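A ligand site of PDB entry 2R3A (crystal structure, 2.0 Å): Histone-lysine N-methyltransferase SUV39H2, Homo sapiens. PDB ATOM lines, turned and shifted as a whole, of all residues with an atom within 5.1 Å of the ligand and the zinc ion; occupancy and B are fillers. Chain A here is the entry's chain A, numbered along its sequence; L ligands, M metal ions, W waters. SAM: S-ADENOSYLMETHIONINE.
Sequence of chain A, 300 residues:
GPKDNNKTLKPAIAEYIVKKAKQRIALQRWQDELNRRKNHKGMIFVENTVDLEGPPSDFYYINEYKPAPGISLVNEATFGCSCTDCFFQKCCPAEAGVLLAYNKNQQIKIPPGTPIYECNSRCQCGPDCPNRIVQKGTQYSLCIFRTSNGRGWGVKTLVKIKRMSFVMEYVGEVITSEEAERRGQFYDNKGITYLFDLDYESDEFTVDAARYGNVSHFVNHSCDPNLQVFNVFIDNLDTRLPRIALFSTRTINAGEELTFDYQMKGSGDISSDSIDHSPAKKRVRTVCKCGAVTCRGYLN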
ATOM      1  N   ARG A 146     -19.283 -24.660 -14.355  1.00  0.00           N
ATOM      2  CA  ARG A 146     -18.045 -24.055 -14.782  1.00  0.00           C
ATOM      3  C   ARG A 146     -17.462 -23.257 -13.601  1.00  0.00           C
ATOM      4  O   ARG A 146     -18.119 -22.347 -13.101  1.00  0.00           O
ATOM      5  CB  ARG A 146     -18.290 -23.134 -15.990  1.00  0.00           C
ATOM      6  CG  ARG A 146     -17.034 -22.685 -16.682  1.00  0.00           C
ATOM      7  CD  ARG A 146     -16.453 -23.812 -17.520  1.00  0.00           C
ATOM      8  NE  ARG A 146     -15.347 -23.326 -18.350  1.00  0.00           N
ATOM      9  CZ  ARG A 146     -14.477 -24.112 -18.974  1.00  0.00           C
ATOM     10  NH1 ARG A 146     -14.541 -25.445 -18.825  1.00  0.00           N
ATOM     11  NH2 ARG A 146     -13.518 -23.572 -19.700  1.00  0.00           N
ATOM     12  N   GLY A 150     -10.713 -20.261 -13.210  1.00  0.00           N
ATOM     13  CA  GLY A 150      -9.813 -20.886 -14.156  1.00  0.00           C
ATOM     14  C   GLY A 150      -9.540 -22.364 -13.969  1.00  0.00           C
ATOM     15  O   GLY A 150      -8.572 -22.860 -14.508  1.00  0.00           O
ATOM     16  N   ARG A 151     -10.407 -23.083 -13.233  1.00  0.00           N
ATOM     17  CA  ARG A 151     -10.196 -24.515 -13.049  1.00  0.00           C
ATOM     18  C   ARG A 151     -11.108 -25.367 -13.975  1.00  0.00           C
ATOM     19  O   ARG A 151     -11.258 -26.569 -13.739  1.00  0.00           O
ATOM     20  CB  ARG A 151     -10.391 -24.908 -11.587  1.00  0.00           C
ATOM     21  CG  ARG A 151      -9.268 -24.400 -10.655  1.00  0.00           C
ATOM     22  CD  ARG A 151      -9.622 -24.606  -9.169  1.00  0.00           C
ATOM     23  NE  ARG A 151     -10.811 -23.827  -8.831  1.00  0.00           N
ATOM     24  CZ  ARG A 151     -11.952 -24.341  -8.372  1.00  0.00           C
ATOM     25  NH1 ARG A 151     -12.087 -25.644  -8.141  1.00  0.00           N
ATOM     26  NH2 ARG A 151     -12.984 -23.528  -8.136  1.00  0.00           N
ATOM     27  N   GLY A 152     -11.691 -24.745 -15.000  1.00  0.00           N
ATOM     28  CA  GLY A 152     -12.520 -25.454 -15.996  1.00  0.00           C
ATOM     29  C   GLY A 152     -13.838 -25.905 -15.369  1.00  0.00           C
ATOM     30  O   GLY A 152     -14.410 -25.192 -14.539  1.00  0.00           O
ATOM     31  N   TRP A 153     -14.334 -27.066 -15.810  1.00  0.00           N
ATOM     32  CA  TRP A 153     -15.482 -27.709 -15.175  1.00  0.00           C
ATOM     33  C   TRP A 153     -15.105 -28.264 -13.820  1.00  0.00           C
ATOM     34  O   TRP A 153     -13.970 -28.702 -13.610  1.00  0.00           O
ATOM     35  CB  TRP A 153     -15.999 -28.870 -16.026  1.00  0.00           C
ATOM     36  CG  TRP A 153     -16.419 -28.463 -17.409  1.00  0.00           C
ATOM     37  CD1 TRP A 153     -15.764 -28.748 -18.572  1.00  0.00           C
ATOM     38  CD2 TRP A 153     -17.568 -27.673 -17.781  1.00  0.00           C
ATOM     39  NE1 TRP A 153     -16.454 -28.201 -19.656  1.00  0.00           N
ATOM     40  CE2 TRP A 153     -17.559 -27.544 -19.188  1.00  0.00           C
ATOM     41  CE3 TRP A 153     -18.623 -27.095 -17.052  1.00  0.00           C
ATOM     42  CZ2 TRP A 153     -18.576 -26.868 -19.884  1.00  0.00           C
ATOM     43  CZ3 TRP A 153     -19.630 -26.436 -17.739  1.00  0.00           C
ATOM     44  CH2 TRP A 153     -19.594 -26.313 -19.145  1.00  0.00           C
ATOM     45  N   GLY A 154     -16.069 -28.213 -12.919  1.00  0.00           N
ATOM     46  CA  GLY A 154     -15.984 -28.911 -11.648  1.00  0.00           C
ATOM     47  C   GLY A 154     -17.314 -29.576 -11.341  1.00  0.00           C
ATOM     48  O   GLY A 154     -18.241 -29.552 -12.165  1.00  0.00           O
ATOM     49  N   ASN A 189      -1.131 -32.230 -19.929  1.00  0.00           N
ATOM     50  CA  ASN A 189      -1.241 -32.344 -18.467  1.00  0.00           C
ATOM     51  C   ASN A 189      -2.601 -32.771 -17.922  1.00  0.00           C
ATOM     52  O   ASN A 189      -2.655 -33.617 -17.038  1.00  0.00           O
ATOM     53  CB  ASN A 189      -0.786 -31.065 -17.767  1.00  0.00           C
ATOM     54  CG  ASN A 189       0.690 -31.088 -17.473  1.00  0.00           C
ATOM     55  OD1 ASN A 189       1.449 -31.765 -18.166  1.00  0.00           O
ATOM     56  ND2 ASN A 189       1.105 -30.371 -16.433  1.00  0.00           N
ATOM     57  N   LYS A 190      -3.653 -32.193 -18.472  1.00  0.00           N
ATOM     58  CA  LYS A 190      -5.041 -32.570 -18.135  1.00  0.00           C
ATOM     59  C   LYS A 190      -5.265 -34.058 -18.418  1.00  0.00           C
ATOM     60  O   LYS A 190      -5.808 -34.755 -17.570  1.00  0.00           O
ATOM     61  CB  LYS A 190      -6.089 -31.657 -18.845  1.00  0.00           C
ATOM     62  CG  LYS A 190      -7.558 -32.039 -18.515  1.00  0.00           C
ATOM     63  CD  LYS A 190      -8.631 -31.060 -19.025  1.00  0.00           C
ATOM     64  CE  LYS A 190      -9.024 -31.419 -20.464  1.00  0.00           C
ATOM     65  NZ  LYS A 190     -10.473 -31.516 -20.636  1.00  0.00           N
ATOM     66  N   THR A 193      -3.928 -36.391 -15.884  1.00  0.00           N
ATOM     67  CA  THR A 193      -4.763 -36.405 -14.664  1.00  0.00           C
ATOM     68  C   THR A 193      -5.903 -37.434 -14.699  1.00  0.00           C
ATOM     69  O   THR A 193      -6.390 -37.841 -13.655  1.00  0.00           O
ATOM     70  CB  THR A 193      -5.340 -34.988 -14.265  1.00  0.00           C
ATOM     71  OG1 THR A 193      -6.301 -34.571 -15.236  1.00  0.00           O
ATOM     72  CG2 THR A 193      -4.223 -33.961 -14.077  1.00  0.00           C
ATOM     73  N   TYR A 194      -6.307 -37.887 -15.892  1.00  0.00           N
ATOM     74  CA  TYR A 194      -7.329 -38.921 -16.006  1.00  0.00           C
ATOM     75  C   TYR A 194      -6.801 -40.350 -15.806  1.00  0.00           C
ATOM     76  O   TYR A 194      -7.591 -41.321 -15.834  1.00  0.00           O
ATOM     77  CB  TYR A 194      -8.036 -38.844 -17.347  1.00  0.00           C
ATOM     78  CG  TYR A 194      -8.696 -37.525 -17.664  1.00  0.00           C
ATOM     79  CD1 TYR A 194      -9.772 -37.042 -16.919  1.00  0.00           C
ATOM     80  CD2 TYR A 194      -8.289 -36.775 -18.759  1.00  0.00           C
ATOM     81  CE1 TYR A 194     -10.401 -35.822 -17.254  1.00  0.00           C
ATOM     82  CE2 TYR A 194      -8.908 -35.545 -19.096  1.00  0.00           C
ATOM     83  CZ  TYR A 194      -9.954 -35.086 -18.334  1.00  0.00           C
ATOM     84  OH  TYR A 194     -10.557 -33.882 -18.671  1.00  0.00           O
ATOM     85  N   HIS A 217     -14.859 -37.836 -13.663  1.00  0.00           N
ATOM     86  CA  HIS A 217     -14.060 -37.261 -14.773  1.00  0.00           C
ATOM     87  C   HIS A 217     -13.996 -35.705 -14.616  1.00  0.00           C
ATOM     88  O   HIS A 217     -13.049 -35.084 -15.086  1.00  0.00           O
ATOM     89  CB  HIS A 217     -14.755 -37.657 -16.116  1.00  0.00           C
ATOM     90  CG  HIS A 217     -14.182 -36.983 -17.347  1.00  0.00           C
ATOM     91  ND1 HIS A 217     -13.204 -37.566 -18.129  1.00  0.00           N
ATOM     92  CD2 HIS A 217     -14.479 -35.799 -17.939  1.00  0.00           C
ATOM     93  CE1 HIS A 217     -12.930 -36.780 -19.156  1.00  0.00           C
ATOM     94  NE2 HIS A 217     -13.689 -35.699 -19.064  1.00  0.00           N
ATOM     95  N   PHE A 218     -14.984 -35.095 -13.956  1.00  0.00           N
ATOM     96  CA  PHE A 218     -15.002 -33.599 -13.854  1.00  0.00           C
ATOM     97  C   PHE A 218     -14.617 -33.048 -12.462  1.00  0.00           C
ATOM     98  O   PHE A 218     -14.612 -31.834 -12.251  1.00  0.00           O
ATOM     99  CB  PHE A 218     -16.365 -33.066 -14.290  1.00  0.00           C
ATOM    100  CG  PHE A 218     -16.711 -33.434 -15.703  1.00  0.00           C
ATOM    101  CD1 PHE A 218     -16.284 -32.645 -16.746  1.00  0.00           C
ATOM    102  CD2 PHE A 218     -17.418 -34.600 -15.988  1.00  0.00           C
ATOM    103  CE1 PHE A 218     -16.600 -32.989 -18.080  1.00  0.00           C
ATOM    104  CE2 PHE A 218     -17.740 -34.939 -17.329  1.00  0.00           C
ATOM    105  CZ  PHE A 218     -17.320 -34.140 -18.344  1.00  0.00           C
ATOM    106  N   VAL A 219     -14.279 -33.946 -11.545  1.00  0.00           N
ATOM    107  CA  VAL A 219     -13.901 -33.538 -10.180  1.00  0.00           C
ATOM    108  C   VAL A 219     -12.504 -32.977 -10.109  1.00  0.00           C
ATOM    109  O   VAL A 219     -11.568 -33.637 -10.532  1.00  0.00           O
ATOM    110  CB  VAL A 219     -14.020 -34.741  -9.187  1.00  0.00           C
ATOM    111  CG1 VAL A 219     -13.481 -34.371  -7.871  1.00  0.00           C
ATOM    112  CG2 VAL A 219     -15.505 -35.112  -9.058  1.00  0.00           C
ATOM    113  N   ASN A 220     -12.393 -31.757  -9.557  1.00  0.00           N
ATOM    114  CA  ASN A 220     -11.100 -31.052  -9.420  1.00  0.00           C
ATOM    115  C   ASN A 220     -10.270 -31.483  -8.208  1.00  0.00           C
ATOM    116  O   ASN A 220     -10.775 -32.089  -7.305  1.00  0.00           O
ATOM    117  CB  ASN A 220     -11.318 -29.527  -9.374  1.00  0.00           C
ATOM    118  CG  ASN A 220     -11.760 -28.969 -10.714  1.00  0.00           C
ATOM    119  OD1 ASN A 220     -12.552 -27.985 -10.804  1.00  0.00           O
ATOM    120  ND2 ASN A 220     -11.248 -29.566 -11.759  1.00  0.00           N
ATOM    121  N   HIS A 221      -8.990 -31.175  -8.270  1.00  0.00           N
ATOM    122  CA  HIS A 221      -8.029 -31.392  -7.200  1.00  0.00           C
ATOM    123  C   HIS A 221      -8.147 -30.342  -6.140  1.00  0.00           C
ATOM    124  O   HIS A 221      -8.277 -29.145  -6.427  1.00  0.00           O
ATOM    125  CB  HIS A 221      -6.608 -31.303  -7.766  1.00  0.00           C
ATOM    126  CG  HIS A 221      -5.565 -31.192  -6.706  1.00  0.00           C
ATOM    127  ND1 HIS A 221      -5.023 -32.294  -6.071  1.00  0.00           N
ATOM    128  CD2 HIS A 221      -5.007 -30.112  -6.121  1.00  0.00           C
ATOM    129  CE1 HIS A 221      -4.163 -31.878  -5.157  1.00  0.00           C
ATOM    130  NE2 HIS A 221      -4.155 -30.565  -5.151  1.00  0.00           N
ATOM    131  N   SER A 222      -8.042 -30.773  -4.894  1.00  0.00           N
ATOM    132  CA  SER A 222      -7.806 -29.830  -3.815  1.00  0.00           C
ATOM    133  C   SER A 222      -6.744 -30.322  -2.864  1.00  0.00           C
ATOM    134  O   SER A 222      -6.619 -31.528  -2.652  1.00  0.00           O
ATOM    135  CB  SER A 222      -9.077 -29.572  -2.998  1.00  0.00           C
ATOM    136  OG  SER A 222      -8.797 -28.785  -1.866  1.00  0.00           O
ATOM    137  N   CYS A 223      -6.034 -29.375  -2.247  1.00  0.00           N
ATOM    138  CA  CYS A 223      -4.997 -29.647  -1.206  1.00  0.00           C
ATOM    139  C   CYS A 223      -5.590 -29.881   0.192  1.00  0.00           C
ATOM    140  O   CYS A 223      -4.898 -30.387   1.122  1.00  0.00           O
ATOM    141  CB  CYS A 223      -3.972 -28.518  -1.197  1.00  0.00           C
ATOM    142  SG  CYS A 223      -3.095 -28.298  -2.810  1.00  0.00           S
ATOM    143  N   TYR A 262      -5.406 -35.263  -5.933  1.00  0.00           N
ATOM    144  CA  TYR A 262      -4.874 -36.015  -7.110  1.00  0.00           C
ATOM    145  C   TYR A 262      -3.589 -36.787  -6.802  1.00  0.00           C
ATOM    146  O   TYR A 262      -3.247 -37.742  -7.511  1.00  0.00           O
ATOM    147  CB  TYR A 262      -4.615 -35.059  -8.297  1.00  0.00           C
ATOM    148  CG  TYR A 262      -5.832 -34.569  -9.068  1.00  0.00           C
ATOM    149  CD1 TYR A 262      -7.142 -34.775  -8.603  1.00  0.00           C
ATOM    150  CD2 TYR A 262      -5.659 -33.820 -10.238  1.00  0.00           C
ATOM    151  CE1 TYR A 262      -8.249 -34.259  -9.307  1.00  0.00           C
ATOM    152  CE2 TYR A 262      -6.743 -33.337 -10.953  1.00  0.00           C
ATOM    153  CZ  TYR A 262      -8.022 -33.570 -10.488  1.00  0.00           C
ATOM    154  OH  TYR A 262      -9.021 -33.064 -11.235  1.00  0.00           O
ATOM    155  N   THR A 286       1.530 -27.718 -13.193  1.00  0.00           N
ATOM    156  CA  THR A 286       0.282 -26.973 -13.225  1.00  0.00           C
ATOM    157  C   THR A 286       0.073 -26.331 -11.871  1.00  0.00           C
ATOM    158  O   THR A 286       0.118 -27.001 -10.829  1.00  0.00           O
ATOM    159  CB  THR A 286      -0.973 -27.894 -13.533  1.00  0.00           C
ATOM    160  OG1 THR A 286      -0.814 -28.545 -14.805  1.00  0.00           O
ATOM    161  CG2 THR A 286      -2.258 -27.078 -13.561  1.00  0.00           C
ATOM    162  N   VAL A 287      -0.181 -25.036 -11.896  1.00  0.00           N
ATOM    163  CA  VAL A 287      -0.370 -24.290 -10.672  1.00  0.00           C
ATOM    164  C   VAL A 287      -1.739 -24.641 -10.070  1.00  0.00           C
ATOM    165  O   VAL A 287      -2.759 -24.654 -10.760  1.00  0.00           O
ATOM    166  CB  VAL A 287      -0.181 -22.755 -10.890  1.00  0.00           C
ATOM    167  CG1 VAL A 287      -0.571 -21.968  -9.653  1.00  0.00           C
ATOM    168  CG2 VAL A 287       1.292 -22.413 -11.325  1.00  0.00           C
ATOM    169  N   CYS A 288      -1.729 -24.961  -8.786  1.00  0.00           N
ATOM    170  CA  CYS A 288      -2.951 -25.275  -8.083  1.00  0.00           C
ATOM    171  C   CYS A 288      -3.717 -24.032  -7.673  1.00  0.00           C
ATOM    172  O   CYS A 288      -3.159 -23.115  -7.030  1.00  0.00           O
ATOM    173  CB  CYS A 288      -2.636 -26.091  -6.840  1.00  0.00           C
ATOM    174  SG  CYS A 288      -4.186 -26.627  -6.138  1.00  0.00           S
ATOM    175  N   LYS A 289      -4.994 -23.984  -8.068  1.00  0.00           N
ATOM    176  CA  LYS A 289      -5.860 -22.858  -7.703  1.00  0.00           C
ATOM    177  C   LYS A 289      -6.979 -23.303  -6.746  1.00  0.00           C
ATOM    178  O   LYS A 289      -8.093 -22.737  -6.714  1.00  0.00           O
ATOM    179  CB  LYS A 289      -6.407 -22.155  -8.977  1.00  0.00           C
ATOM    180  CG  LYS A 289      -5.284 -21.574  -9.894  1.00  0.00           C
ATOM    181  CD  LYS A 289      -5.823 -20.688 -11.012  1.00  0.00           C
ATOM    182  CE  LYS A 289      -6.284 -19.314 -10.404  1.00  0.00           C
ATOM    183  NZ  LYS A 289      -6.479 -18.205 -11.415  1.00  0.00           N
ATOM    184  N   CYS A 290      -6.671 -24.305  -5.928  1.00  0.00           N
ATOM    185  CA  CYS A 290      -7.711 -24.885  -5.068  1.00  0.00           C
ATOM    186  C   CYS A 290      -8.256 -23.887  -4.047  1.00  0.00           C
ATOM    187  O   CYS A 290      -9.404 -24.012  -3.599  1.00  0.00           O
ATOM    188  CB  CYS A 290      -7.258 -26.209  -4.406  1.00  0.00           C
ATOM    189  SG  CYS A 290      -6.132 -26.037  -2.922  1.00  0.00           S
ATOM    190  N   GLY A 291      -7.435 -22.890  -3.689  1.00  0.00           N
ATOM    191  CA  GLY A 291      -7.850 -21.816  -2.780  1.00  0.00           C
ATOM    192  C   GLY A 291      -7.661 -22.053  -1.291  1.00  0.00           C
ATOM    193  O   GLY A 291      -7.960 -21.178  -0.479  1.00  0.00           O
ATOM    194  N   CYS A 295      -2.727 -24.581   0.555  1.00  0.00           N
ATOM    195  CA  CYS A 295      -2.475 -24.985  -0.817  1.00  0.00           C
ATOM    196  C   CYS A 295      -0.981 -25.304  -1.056  1.00  0.00           C
ATOM    197  O   CYS A 295      -0.099 -24.554  -0.630  1.00  0.00           O
ATOM    198  CB  CYS A 295      -2.962 -23.914  -1.803  1.00  0.00           C
ATOM    199  SG  CYS A 295      -2.667 -24.375  -3.516  1.00  0.00           S
ATOM    200  N   ARG A 296      -0.702 -26.419  -1.738  1.00  0.00           N
ATOM    201  CA  ARG A 296       0.699 -26.809  -1.984  1.00  0.00           C
ATOM    202  C   ARG A 296       1.319 -26.107  -3.196  1.00  0.00           C
ATOM    203  O   ARG A 296       2.552 -26.189  -3.435  1.00  0.00           O
ATOM    204  CB  ARG A 296       0.835 -28.325  -2.086  1.00  0.00           C
ATOM    205  CG  ARG A 296       0.242 -29.072  -0.883  1.00  0.00           C
ATOM    206  CD  ARG A 296       0.574 -30.562  -0.904  1.00  0.00           C
ATOM    207  NE  ARG A 296       0.110 -31.279  -2.110  1.00  0.00           N
ATOM    208  CZ  ARG A 296      -0.990 -32.042  -2.174  1.00  0.00           C
ATOM    209  NH1 ARG A 296      -1.766 -32.203  -1.115  1.00  0.00           N
ATOM    210  NH2 ARG A 296      -1.272 -32.665  -3.317  1.00  0.00           N
ATOM    211  N   GLY A 297       0.469 -25.453  -3.979  1.00  0.00           N
ATOM    212  CA  GLY A 297       0.905 -24.564  -5.069  1.00  0.00           C
ATOM    213  C   GLY A 297       0.849 -25.198  -6.435  1.00  0.00           C
ATOM    214  O   GLY A 297       0.736 -24.502  -7.459  1.00  0.00           O
ATOM    215  N   LEU A 299      -0.314 -28.998  -8.778  1.00  0.00           N
ATOM    216  CA  LEU A 299      -1.022 -30.293  -8.864  1.00  0.00           C
ATOM    217  C   LEU A 299      -0.066 -31.485  -9.009  1.00  0.00           C
ATOM    218  O   LEU A 299      -0.389 -32.588  -8.542  1.00  0.00           O
ATOM    219  CB  LEU A 299      -2.043 -30.325 -10.026  1.00  0.00           C
ATOM    220  CG  LEU A 299      -3.104 -29.240 -10.227  1.00  0.00           C
ATOM    221  CD1 LEU A 299      -4.172 -29.734 -11.184  1.00  0.00           C
ATOM    222  CD2 LEU A 299      -3.738 -28.858  -8.945  1.00  0.00           C
HETATM  223  N   SAM L   1     -11.411 -29.057 -14.563  1.00  0.00           N
HETATM  224  CA  SAM L   1     -11.526 -30.266 -15.417  1.00  0.00           C
HETATM  225  C   SAM L   1     -12.301 -29.987 -16.730  1.00  0.00           C
HETATM  226  O   SAM L   1     -12.593 -28.855 -17.078  1.00  0.00           O
HETATM  227  OXT SAM L   1     -12.666 -30.872 -17.463  1.00  0.00           O
HETATM  228  CB  SAM L   1     -12.069 -31.443 -14.623  1.00  0.00           C
HETATM  229  CG  SAM L   1     -11.001 -32.243 -13.875  1.00  0.00           C
HETATM  230  SD  SAM L   1      -9.643 -32.878 -14.922  1.00  0.00           S
HETATM  231  CE  SAM L   1      -9.691 -34.543 -14.185  1.00  0.00           C
HETATM  232  C5' SAM L   1      -8.143 -32.163 -14.162  1.00  0.00           C
HETATM  233  C4' SAM L   1      -7.748 -30.813 -14.772  1.00  0.00           C
HETATM  234  O4' SAM L   1      -8.577 -29.782 -14.249  1.00  0.00           O
HETATM  235  C3' SAM L   1      -6.328 -30.375 -14.503  1.00  0.00           C
HETATM  236  O3' SAM L   1      -5.407 -30.758 -15.492  1.00  0.00           O
HETATM  237  C2' SAM L   1      -6.462 -28.864 -14.482  1.00  0.00           C
HETATM  238  O2' SAM L   1      -6.578 -28.366 -15.794  1.00  0.00           O
HETATM  239  C1' SAM L   1      -7.835 -28.636 -13.890  1.00  0.00           C
HETATM  240  N9  SAM L   1      -7.753 -28.556 -12.413  1.00  0.00           N
HETATM  241  C8  SAM L   1      -8.306 -29.427 -11.504  1.00  0.00           C
HETATM  242  N7  SAM L   1      -8.019 -29.005 -10.272  1.00  0.00           N
HETATM  243  C5  SAM L   1      -7.320 -27.873 -10.357  1.00  0.00           C
HETATM  244  C6  SAM L   1      -6.754 -27.009  -9.399  1.00  0.00           C
HETATM  245  N6  SAM L   1      -6.892 -27.228  -8.083  1.00  0.00           N
HETATM  246  N1  SAM L   1      -6.057 -25.909  -9.859  1.00  0.00           N
HETATM  247  C2  SAM L   1      -5.893 -25.640 -11.195  1.00  0.00           C
HETATM  248  N3  SAM L   1      -6.462 -26.479 -12.134  1.00  0.00           N
HETATM  249  C4  SAM L   1      -7.136 -27.578 -11.709  1.00  0.00           C
HETATM  250 ZN    ZN M   1      -4.018 -26.326  -3.825  1.00  0.00          ZN
HETATM  251  O   HOH W   1     -12.552 -27.482 -19.464  1.00  0.00           O
HETATM  252  O   HOH W   2     -12.807 -33.302 -17.506  1.00  0.00           O
HETATM  253  O   HOH W   3      -2.994 -30.509 -14.919  1.00  0.00           O
HETATM  254  O   HOH W   4      -5.692 -25.381 -14.617  1.00  0.00           O
HETATM  255  O   HOH W   5      -9.587 -27.557 -16.566  1.00  0.00           O
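OXT of the ligand is in salt-bridge range of NZ of Lys 190. A nitrogen (N) of the ligand sits at hydrogen-bond distance from the backbone carbonyl oxygen of Trp 153 (2.8 Å). The backbone carbonyl oxygen (O) of Arg 151 lies within hydrogen-bond range of a nitrogen (N) of the ligand, at 2.6 Å. N of Trp 153 is in hydrogen-bond range of O of the ligand, at 2.8 Å. The side-chain sulfur (SG) of Cys 288 sits close to a nitrogen (N6) of the ligand. The backbone carbonyl oxygen of His 221 sits at hydrogen-bond distance from a nitrogen (N6) of the ligand (2.9 Å). The backbone NH of Lys 289 lies within hydrogen-bond range of a nitrogen (N1) of the ligand, at 2.8 Å. A nitrogen (N7) of the ligand is in hydrogen-bond range of the backbone NH (N) of His 221, at 3.1 Å. The side-chain amide nitrogen (ND2) of Asn 220 sits close to a nitrogen (N) of the ligand.
The backbone NH of Cys 288 is in hydrogen-bond range of the backbone carbonyl oxygen of Gly 297, 2.8 Å away. The side-chain sulfur (SG) of Cys 223 sits close to a ring nitrogen (NE2) of His 221 (3.4 Å). The side-chain sulfur of Cys 295 sits close to the backbone NH of Gly 297, at 3.3 Å. The side-chain amino group (NZ) of Lys 190 sits at hydrogen-bond distance from the side-chain hydroxyl (OH) of Tyr 194. The backbone carbonyl oxygen (O) of Trp 153 sits close to the side-chain amide oxygen (OD1) of Asn 220, at 3.2 Å. The backbone carbonyl oxygen (O) of Thr 286 sits at hydrogen-bond distance from the backbone NH (N) of Leu 299 (2.9 Å). O of Val 219 lies within hydrogen-bond range of OH of Tyr 262 (2.7 Å). The backbone NH (N) of Arg 296 sits close to the side-chain sulfur (SG) of Cys 223 (3.2 Å).
The side-chain hydroxyl (OG1) of Thr 193 lies close to a sulfur (SD) of the ligand. OH of Tyr 262 lies close to SD of the ligand (3.7 Å). Gly 152 touches the ligand. Tyr 194 touches the ligand (CE1 to CE, 3.4 Å). His 217 touches the ligand (O to CE, 3.5 Å). O of Phe 218 touches CB of the ligand, 3.5 Å away. Val 219 touches the ligand (O to CG, 3.7 Å). Val 287 touches the ligand. Leu 299 touches the ligand. Hydrophobic or aromatic side chains within 4 Å of the ligand: Trp 153, Tyr 194, His 221, Tyr 262 and Leu 299. Of the 28 residues printed, 17 come within 4 Å of the ligand. The nearest printed residue that does not touch the ligand is Asn 189 (4.2 Å).
Residues that only touch the zinc ion: Arg 296 (3.9 Å). Five residues have an atom within 4 Å of the zinc ion: Cys 223, Cys 288, Cys 290, Cys 295 and Arg 296. The nearest printed residue that does not touch the zinc ion is His 221 (4.4 Å).
The zinc ion is bound by SG of Cys 290, 2.3 Å away. The zinc ion is bound by SG of Cys 288, 2.3 Å away. The zinc ion is bound by the side-chain sulfur (SG) of Cys 295 (2.4 Å). SG of Cys 223 is bound to the zinc ion, at 2.4 Å.
Water W2 lies within hydrogen-bond range of OXT of the ligand, OH of Tyr 194 and NE2 of His 217. Water W3 bridges an oxygen (O3') of the ligand (2.5 Å) and the side-chain hydroxyl of Thr 286 (2.9 Å). Water W1 bridges an oxygen (O) of the ligand (2.8 Å) and the guanidinium group of Arg 146 (2.9 Å). Water W5 lies within hydrogen-bond range of a nitrogen (N) of the ligand (3.1 Å) and the backbone carbonyl oxygen of Arg 151 (3.4 Å).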
